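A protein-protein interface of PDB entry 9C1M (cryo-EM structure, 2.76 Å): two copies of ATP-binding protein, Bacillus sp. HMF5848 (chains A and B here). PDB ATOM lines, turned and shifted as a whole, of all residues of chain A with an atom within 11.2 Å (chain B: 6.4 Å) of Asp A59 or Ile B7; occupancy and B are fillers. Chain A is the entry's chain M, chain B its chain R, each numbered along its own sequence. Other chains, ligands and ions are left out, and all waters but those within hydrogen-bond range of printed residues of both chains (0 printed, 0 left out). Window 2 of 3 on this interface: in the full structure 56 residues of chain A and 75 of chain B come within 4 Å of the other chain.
Among the printed residues, merely in contact across the chains: Lys A55 with Glu B8, Ile A56 with Glu B8, Ser A57 with Ile B7, Ser A57 with Glu B8, Thr A58 with Pro B90 and Asp A59 with Ile B7.
No position is printed for both chains.
Of the 8 pairs that touch across the chains among the printed residues, none has its exchanged pair printed and touching as well.
Printed residues of chain B within 4 Å of Ser A57: Ile B7 (3.9 Å) and Glu B8 (3.7 Å).
Of the printed residues of chain B, Thr A58 touches Ile B7 (3.2 Å) and Pro B90 (3.1 Å).
Of chain B, only Ile B7 comes within 4 Å of Asp A59.
Asp A61 touches none of the printed residues of chain B.
No residue of chain A comes within 4 Å of Ser B5.
Ile B7 touches just these residues of chain A: Ser A57 (3.9 Å), Thr A58 (3.2 Å) and Asp A59 (3.3 Å).
Of the printed residues of chain A, Ser B9 touches Ile A56 (3.1 Å).
No residue of chain A comes within 4 Å of Leu B15.
No residue of chain A comes within 4 Å of Lys B17.
Ile B66 touches none of the printed residues of chain A.
Of chain A, only Thr A58 comes within 4 Å of Pro B90.
The nearest residue of chain A that does not touch Ile B7 is Ile A56 (4.6 Å).
The nearest printed residue of chain B that does not touch Thr A58 is Thr B91 (4.6 Å).
O of Ile A56 lies within hydrogen-bond range of N of Ser B9 (3.1 Å).
O of Ile B7 lies within hydrogen-bond range of N of Thr A58 (3.2 Å).
Hydrophobic or aromatic side chains of chain A that line the printed part of chain B: Ile A56.
Of the 13 printed residues of chain B, 4 touch a printed residue of chain A.
Printed residues of chain B that touch a printed residue of chain A: Ile B7, Glu B8, Ser B9 and Pro B90.
Hydrophobic or aromatic side chains of chain B within 4 Å of the printed part of chain A: Ile B7 and Pro B90.
Along chain B the printed residues that touch a printed residue of chain A span positions 7 to 90.
Among the printed residues, no Asp or Glu carboxylate lies within 4 Å of a Lys or Arg side-chain nitrogen of the other chain.
The backbone carbonyl oxygen (O) of Glu A62 sits close to the backbone carbonyl oxygen (O) of Ser A57 (2.7 Å).
The backbone carbonyl oxygen (O) of Ser A57 is in hydrogen-bond range of the backbone NH (N) of Ile A64, at 2.8 Å.
OG1 of Thr A58 lies close to OD1 of Asp A63 (3.5 Å).
The backbone NH (N) of Ile B7 is in hydrogen-bond range of the backbone carbonyl oxygen (O) of Leu B15 (3.0 Å).
The backbone NH (N) of Leu B15 sits at hydrogen-bond distance from the backbone carbonyl oxygen (O) of Glu B8 (2.6 Å).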
ATOM      1  N   LEU A  21     -13.867 -19.087  39.206  1.00  0.00           N
ATOM      2  CA  LEU A  21     -13.149 -19.483  37.998  1.00  0.00           C
ATOM      3  C   LEU A  21     -11.749 -19.994  38.317  1.00  0.00           C
ATOM      4  O   LEU A  21     -11.290 -20.974  37.718  1.00  0.00           O
ATOM      5  CB  LEU A  21     -13.078 -18.308  37.023  1.00  0.00           C
ATOM      6  CG  LEU A  21     -12.373 -18.565  35.690  1.00  0.00           C
ATOM      7  CD1 LEU A  21     -13.194 -19.491  34.810  1.00  0.00           C
ATOM      8  CD2 LEU A  21     -12.085 -17.254  34.973  1.00  0.00           C
ATOM      9  N   ILE A  54     -19.874 -32.262  32.603  1.00  0.00           N
ATOM     10  CA  ILE A  54     -19.412 -30.940  33.001  1.00  0.00           C
ATOM     11  C   ILE A  54     -19.994 -29.924  32.029  1.00  0.00           C
ATOM     12  O   ILE A  54     -20.274 -30.235  30.869  1.00  0.00           O
ATOM     13  CB  ILE A  54     -17.868 -30.861  33.048  1.00  0.00           C
ATOM     14  CG1 ILE A  54     -17.293 -32.164  33.615  1.00  0.00           C
ATOM     15  CG2 ILE A  54     -17.411 -29.667  33.866  1.00  0.00           C
ATOM     16  CD1 ILE A  54     -15.803 -32.326  33.450  1.00  0.00           C
ATOM     17  N   LYS A  55     -20.199 -28.701  32.517  1.00  0.00           N
ATOM     18  CA  LYS A  55     -20.890 -27.681  31.733  1.00  0.00           C
ATOM     19  C   LYS A  55     -20.469 -26.316  32.257  1.00  0.00           C
ATOM     20  O   LYS A  55     -20.897 -25.917  33.345  1.00  0.00           O
ATOM     21  CB  LYS A  55     -22.400 -27.873  31.835  1.00  0.00           C
ATOM     22  CG  LYS A  55     -23.249 -26.905  31.026  1.00  0.00           C
ATOM     23  CD  LYS A  55     -23.082 -27.112  29.534  1.00  0.00           C
ATOM     24  CE  LYS A  55     -23.928 -26.122  28.747  1.00  0.00           C
ATOM     25  NZ  LYS A  55     -25.384 -26.354  28.940  1.00  0.00           N
ATOM     26  N   ILE A  56     -19.642 -25.606  31.495  1.00  0.00           N
ATOM     27  CA  ILE A  56     -19.203 -24.261  31.852  1.00  0.00           C
ATOM     28  C   ILE A  56     -19.795 -23.289  30.837  1.00  0.00           C
ATOM     29  O   ILE A  56     -19.606 -23.448  29.624  1.00  0.00           O
ATOM     30  CB  ILE A  56     -17.669 -24.157  31.926  1.00  0.00           C
ATOM     31  CG1 ILE A  56     -17.008 -24.584  30.614  1.00  0.00           C
ATOM     32  CG2 ILE A  56     -17.140 -25.016  33.061  1.00  0.00           C
ATOM     33  CD1 ILE A  56     -15.499 -24.713  30.706  1.00  0.00           C
ATOM     34  N   SER A  57     -20.537 -22.301  31.332  1.00  0.00           N
ATOM     35  CA  SER A  57     -21.262 -21.375  30.477  1.00  0.00           C
ATOM     36  C   SER A  57     -21.114 -19.957  31.004  1.00  0.00           C
ATOM     37  O   SER A  57     -21.184 -19.725  32.214  1.00  0.00           O
ATOM     38  CB  SER A  57     -22.749 -21.745  30.391  1.00  0.00           C
ATOM     39  OG  SER A  57     -22.917 -23.139  30.203  1.00  0.00           O
ATOM     40  N   THR A  58     -20.899 -19.015  30.089  1.00  0.00           N
ATOM     41  CA  THR A  58     -20.823 -17.590  30.407  1.00  0.00           C
ATOM     42  C   THR A  58     -21.620 -16.792  29.376  1.00  0.00           C
ATOM     43  O   THR A  58     -21.137 -15.831  28.778  1.00  0.00           O
ATOM     44  CB  THR A  58     -19.370 -17.121  30.493  1.00  0.00           C
ATOM     45  OG1 THR A  58     -18.626 -18.040  31.301  1.00  0.00           O
ATOM     46  CG2 THR A  58     -19.280 -15.734  31.121  1.00  0.00           C
ATOM     47  N   ASP A  59     -22.856 -17.217  29.132  1.00  0.00           N
ATOM     48  CA  ASP A  59     -23.736 -16.484  28.234  1.00  0.00           C
ATOM     49  C   ASP A  59     -24.371 -15.313  28.972  1.00  0.00           C
ATOM     50  O   ASP A  59     -24.965 -15.489  30.041  1.00  0.00           O
ATOM     51  CB  ASP A  59     -24.814 -17.408  27.669  1.00  0.00           C
ATOM     52  CG  ASP A  59     -24.267 -18.380  26.643  1.00  0.00           C
ATOM     53  OD1 ASP A  59     -23.571 -17.931  25.708  1.00  0.00           O
ATOM     54  OD2 ASP A  59     -24.533 -19.595  26.770  1.00  0.00           O
ATOM     55  N   LYS A  60     -24.236 -14.115  28.397  1.00  0.00           N
ATOM     56  CA  LYS A  60     -24.818 -12.889  28.947  1.00  0.00           C
ATOM     57  C   LYS A  60     -24.307 -12.608  30.362  1.00  0.00           C
ATOM     58  O   LYS A  60     -25.076 -12.308  31.278  1.00  0.00           O
ATOM     59  CB  LYS A  60     -26.348 -12.949  28.917  1.00  0.00           C
ATOM     60  CG  LYS A  60     -27.016 -11.612  28.640  1.00  0.00           C
ATOM     61  CD  LYS A  60     -28.530 -11.736  28.675  1.00  0.00           C
ATOM     62  CE  LYS A  60     -29.198 -10.375  28.571  1.00  0.00           C
ATOM     63  NZ  LYS A  60     -29.023  -9.575  29.814  1.00  0.00           N
ATOM     64  N   ASP A  61     -22.986 -12.708  30.530  1.00  0.00           N
ATOM     65  CA  ASP A  61     -22.309 -12.369  31.785  1.00  0.00           C
ATOM     66  C   ASP A  61     -22.866 -13.173  32.960  1.00  0.00           C
ATOM     67  O   ASP A  61     -23.237 -12.624  34.000  1.00  0.00           O
ATOM     68  CB  ASP A  61     -22.391 -10.866  32.064  1.00  0.00           C
ATOM     69  CG  ASP A  61     -21.417 -10.062  31.226  1.00  0.00           C
ATOM     70  OD1 ASP A  61     -20.298 -10.554  30.978  1.00  0.00           O
ATOM     71  OD2 ASP A  61     -21.773  -8.937  30.818  1.00  0.00           O
ATOM     72  N   GLU A  62     -22.923 -14.493  32.787  1.00  0.00           N
ATOM     73  CA  GLU A  62     -23.438 -15.405  33.810  1.00  0.00           C
ATOM     74  C   GLU A  62     -22.460 -16.571  33.934  1.00  0.00           C
ATOM     75  O   GLU A  62     -22.546 -17.547  33.186  1.00  0.00           O
ATOM     76  CB  GLU A  62     -24.849 -15.874  33.457  1.00  0.00           C
ATOM     77  CG  GLU A  62     -25.434 -16.890  34.423  1.00  0.00           C
ATOM     78  CD  GLU A  62     -26.238 -16.247  35.535  1.00  0.00           C
ATOM     79  OE1 GLU A  62     -26.246 -15.002  35.622  1.00  0.00           O
ATOM     80  OE2 GLU A  62     -26.863 -16.989  36.322  1.00  0.00           O
ATOM     81  N   ASP A  63     -21.530 -16.464  34.884  1.00  0.00           N
ATOM     82  CA  ASP A  63     -20.531 -17.505  35.111  1.00  0.00           C
ATOM     83  C   ASP A  63     -21.195 -18.721  35.745  1.00  0.00           C
ATOM     84  O   ASP A  63     -21.574 -18.690  36.920  1.00  0.00           O
ATOM     85  CB  ASP A  63     -19.412 -16.975  36.004  1.00  0.00           C
ATOM     86  CG  ASP A  63     -18.560 -15.926  35.316  1.00  0.00           C
ATOM     87  OD1 ASP A  63     -18.435 -15.980  34.078  1.00  0.00           O
ATOM     88  OD2 ASP A  63     -18.015 -15.046  36.014  1.00  0.00           O
ATOM     89  N   ILE A  64     -21.331 -19.798  34.973  1.00  0.00           N
ATOM     90  CA  ILE A  64     -21.949 -21.034  35.438  1.00  0.00           C
ATOM     91  C   ILE A  64     -20.956 -22.173  35.263  1.00  0.00           C
ATOM     92  O   ILE A  64     -20.409 -22.364  34.170  1.00  0.00           O
ATOM     93  CB  ILE A  64     -23.260 -21.334  34.688  1.00  0.00           C
ATOM     94  CG1 ILE A  64     -24.255 -20.190  34.878  1.00  0.00           C
ATOM     95  CG2 ILE A  64     -23.860 -22.644  35.163  1.00  0.00           C
ATOM     96  CD1 ILE A  64     -24.646 -19.957  36.322  1.00  0.00           C
ATOM     97  N   PHE A  65     -20.726 -22.924  36.337  1.00  0.00           N
ATOM     98  CA  PHE A  65     -19.881 -24.117  36.321  1.00  0.00           C
ATOM     99  C   PHE A  65     -20.643 -25.203  37.077  1.00  0.00           C
ATOM    100  O   PHE A  65     -20.582 -25.267  38.308  1.00  0.00           O
ATOM    101  CB  PHE A  65     -18.509 -23.862  36.948  1.00  0.00           C
ATOM    102  CG  PHE A  65     -17.840 -22.591  36.486  1.00  0.00           C
ATOM    103  CD1 PHE A  65     -18.245 -21.353  36.964  1.00  0.00           C
ATOM    104  CD2 PHE A  65     -16.800 -22.637  35.574  1.00  0.00           C
ATOM    105  CE1 PHE A  65     -17.628 -20.193  36.537  1.00  0.00           C
ATOM    106  CE2 PHE A  65     -16.181 -21.481  35.143  1.00  0.00           C
ATOM    107  CZ  PHE A  65     -16.595 -20.258  35.627  1.00  0.00           C
ATOM    108  N   SER B   5     -14.701 -15.706  20.336  1.00  0.00           N
ATOM    109  CA  SER B   5     -14.511 -16.073  21.731  1.00  0.00           C
ATOM    110  C   SER B   5     -15.414 -17.251  22.069  1.00  0.00           C
ATOM    111  O   SER B   5     -16.366 -17.558  21.348  1.00  0.00           O
ATOM    112  CB  SER B   5     -14.802 -14.895  22.671  1.00  0.00           C
ATOM    113  OG  SER B   5     -16.138 -14.445  22.525  1.00  0.00           O
ATOM    114  N   VAL B   6     -15.103 -17.908  23.181  1.00  0.00           N
ATOM    115  CA  VAL B   6     -15.846 -19.078  23.632  1.00  0.00           C
ATOM    116  C   VAL B   6     -16.942 -18.635  24.591  1.00  0.00           C
ATOM    117  O   VAL B   6     -16.677 -17.933  25.573  1.00  0.00           O
ATOM    118  CB  VAL B   6     -14.909 -20.098  24.301  1.00  0.00           C
ATOM    119  CG1 VAL B   6     -15.710 -21.231  24.918  1.00  0.00           C
ATOM    120  CG2 VAL B   6     -13.909 -20.635  23.295  1.00  0.00           C
ATOM    121  N   ILE B   7     -18.175 -19.045  24.306  1.00  0.00           N
ATOM    122  CA  ILE B   7     -19.305 -18.750  25.175  1.00  0.00           C
ATOM    123  C   ILE B   7     -19.760 -19.963  25.977  1.00  0.00           C
ATOM    124  O   ILE B   7     -20.482 -19.789  26.970  1.00  0.00           O
ATOM    125  CB  ILE B   7     -20.490 -18.173  24.375  1.00  0.00           C
ATOM    126  CG1 ILE B   7     -20.915 -19.152  23.278  1.00  0.00           C
ATOM    127  CG2 ILE B   7     -20.126 -16.823  23.785  1.00  0.00           C
ATOM    128  CD1 ILE B   7     -22.328 -18.944  22.785  1.00  0.00           C
ATOM    129  N   GLU B   8     -19.367 -21.172  25.586  1.00  0.00           N
ATOM    130  CA  GLU B   8     -19.801 -22.387  26.264  1.00  0.00           C
ATOM    131  C   GLU B   8     -18.867 -23.525  25.889  1.00  0.00           C
ATOM    132  O   GLU B   8     -18.568 -23.718  24.706  1.00  0.00           O
ATOM    133  CB  GLU B   8     -21.249 -22.734  25.898  1.00  0.00           C
ATOM    134  CG  GLU B   8     -21.849 -23.845  26.736  1.00  0.00           C
ATOM    135  CD  GLU B   8     -21.475 -25.220  26.210  1.00  0.00           C
ATOM    136  OE1 GLU B   8     -21.251 -25.343  24.987  1.00  0.00           O
ATOM    137  OE2 GLU B   8     -21.370 -26.165  27.015  1.00  0.00           O
ATOM    138  N   SER B   9     -18.417 -24.276  26.891  1.00  0.00           N
ATOM    139  CA  SER B   9     -17.577 -25.446  26.679  1.00  0.00           C
ATOM    140  C   SER B   9     -18.190 -26.638  27.397  1.00  0.00           C
ATOM    141  O   SER B   9     -18.527 -26.552  28.580  1.00  0.00           O
ATOM    142  CB  SER B   9     -16.149 -25.206  27.169  1.00  0.00           C
ATOM    143  OG  SER B   9     -15.538 -24.141  26.461  1.00  0.00           O
ATOM    144  N   ILE B  14     -18.161 -27.343  22.005  1.00  0.00           N
ATOM    145  CA  ILE B  14     -17.715 -26.027  22.442  1.00  0.00           C
ATOM    146  C   ILE B  14     -18.364 -24.988  21.541  1.00  0.00           C
ATOM    147  O   ILE B  14     -18.251 -25.071  20.313  1.00  0.00           O
ATOM    148  CB  ILE B  14     -16.180 -25.895  22.403  1.00  0.00           C
ATOM    149  CG1 ILE B  14     -15.535 -26.769  23.480  1.00  0.00           C
ATOM    150  CG2 ILE B  14     -15.761 -24.444  22.567  1.00  0.00           C
ATOM    151  CD1 ILE B  14     -14.135 -27.228  23.135  1.00  0.00           C
ATOM    152  N   LEU B  15     -19.038 -24.014  22.144  1.00  0.00           N
ATOM    153  CA  LEU B  15     -19.736 -22.970  21.406  1.00  0.00           C
ATOM    154  C   LEU B  15     -18.859 -21.728  21.322  1.00  0.00           C
ATOM    155  O   LEU B  15     -18.300 -21.286  22.331  1.00  0.00           O
ATOM    156  CB  LEU B  15     -21.074 -22.637  22.067  1.00  0.00           C
ATOM    157  CG  LEU B  15     -22.119 -23.755  22.048  1.00  0.00           C
ATOM    158  CD1 LEU B  15     -23.349 -23.364  22.852  1.00  0.00           C
ATOM    159  CD2 LEU B  15     -22.498 -24.109  20.620  1.00  0.00           C
ATOM    160  N   VAL B  16     -18.744 -21.169  20.118  1.00  0.00           N
ATOM    161  CA  VAL B  16     -17.862 -20.041  19.845  1.00  0.00           C
ATOM    162  C   VAL B  16     -18.684 -18.921  19.221  1.00  0.00           C
ATOM    163  O   VAL B  16     -19.479 -19.164  18.306  1.00  0.00           O
ATOM    164  CB  VAL B  16     -16.698 -20.442  18.918  1.00  0.00           C
ATOM    165  CG1 VAL B  16     -15.951 -19.214  18.424  1.00  0.00           C
ATOM    166  CG2 VAL B  16     -15.755 -21.394  19.637  1.00  0.00           C
ATOM    167  N   LYS B  17     -18.494 -17.700  19.716  1.00  0.00           N
ATOM    168  CA  LYS B  17     -19.197 -16.522  19.228  1.00  0.00           C
ATOM    169  C   LYS B  17     -18.257 -15.681  18.376  1.00  0.00           C
ATOM    170  O   LYS B  17     -17.156 -15.335  18.817  1.00  0.00           O
ATOM    171  CB  LYS B  17     -19.737 -15.688  20.391  1.00  0.00           C
ATOM    172  CG  LYS B  17     -20.537 -14.467  19.971  1.00  0.00           C
ATOM    173  CD  LYS B  17     -21.130 -13.761  21.180  1.00  0.00           C
ATOM    174  CE  LYS B  17     -21.803 -12.457  20.784  1.00  0.00           C
ATOM    175  NZ  LYS B  17     -22.996 -12.687  19.926  1.00  0.00           N
ATOM    176  N   ILE B  66     -22.876 -17.985  15.882  1.00  0.00           N
ATOM    177  CA  ILE B  66     -22.570 -19.060  16.817  1.00  0.00           C
ATOM    178  C   ILE B  66     -22.000 -20.240  16.044  1.00  0.00           C
ATOM    179  O   ILE B  66     -22.578 -20.670  15.038  1.00  0.00           O
ATOM    180  CB  ILE B  66     -23.816 -19.474  17.619  1.00  0.00           C
ATOM    181  CG1 ILE B  66     -24.415 -18.256  18.325  1.00  0.00           C
ATOM    182  CG2 ILE B  66     -23.468 -20.561  18.624  1.00  0.00           C
ATOM    183  CD1 ILE B  66     -23.628 -17.794  19.531  1.00  0.00           C
ATOM    184  N   PRO B  90     -14.519 -20.296  29.295  1.00  0.00           N
ATOM    185  CA  PRO B  90     -15.256 -19.347  28.456  1.00  0.00           C
ATOM    186  C   PRO B  90     -14.476 -18.062  28.235  1.00  0.00           C
ATOM    187  O   PRO B  90     -13.560 -17.714  28.984  1.00  0.00           O
ATOM    188  CB  PRO B  90     -16.536 -19.087  29.255  1.00  0.00           C
ATOM    189  CG  PRO B  90     -16.690 -20.292  30.118  1.00  0.00           C
ATOM    190  CD  PRO B  90     -15.294 -20.693  30.483  1.00  0.00           C
ATOM    191  N   THR B  91     -14.854 -17.359  27.165  1.00  0.00           N
ATOM    192  CA  THR B  91     -14.242 -16.104  26.728  1.00  0.00           C
ATOM    193  C   THR B  91     -12.778 -16.273  26.333  1.00  0.00           C
ATOM    194  O   THR B  91     -12.038 -15.288  26.246  1.00  0.00           O
ATOM    195  CB  THR B  91     -14.378 -15.001  27.789  1.00  0.00           C
ATOM    196  OG1 THR B  91     -13.617 -15.347  28.953  1.00  0.00           O
ATOM    197  CG2 THR B  91     -15.836 -14.820  28.177  1.00  0.00           C
ATOM    198  N   GLU B  92     -12.341 -17.507  26.089  1.00  0.00           N
ATOM    199  CA  GLU B  92     -11.004 -17.718  25.553  1.00  0.00           C
ATOM    200  C   GLU B  92     -10.986 -17.402  24.058  1.00  0.00           C
ATOM    201  O   GLU B  92     -11.933 -17.738  23.341  1.00  0.00           O
ATOM    202  CB  GLU B  92     -10.544 -19.156  25.786  1.00  0.00           C
ATOM    203  CG  GLU B  92     -10.096 -19.442  27.212  1.00  0.00           C
ATOM    204  CD  GLU B  92      -8.623 -19.163  27.432  1.00  0.00           C
ATOM    205  OE1 GLU B  92      -7.987 -18.568  26.537  1.00  0.00           O
ATOM    206  OE2 GLU B  92      -8.099 -19.539  28.502  1.00  0.00           O
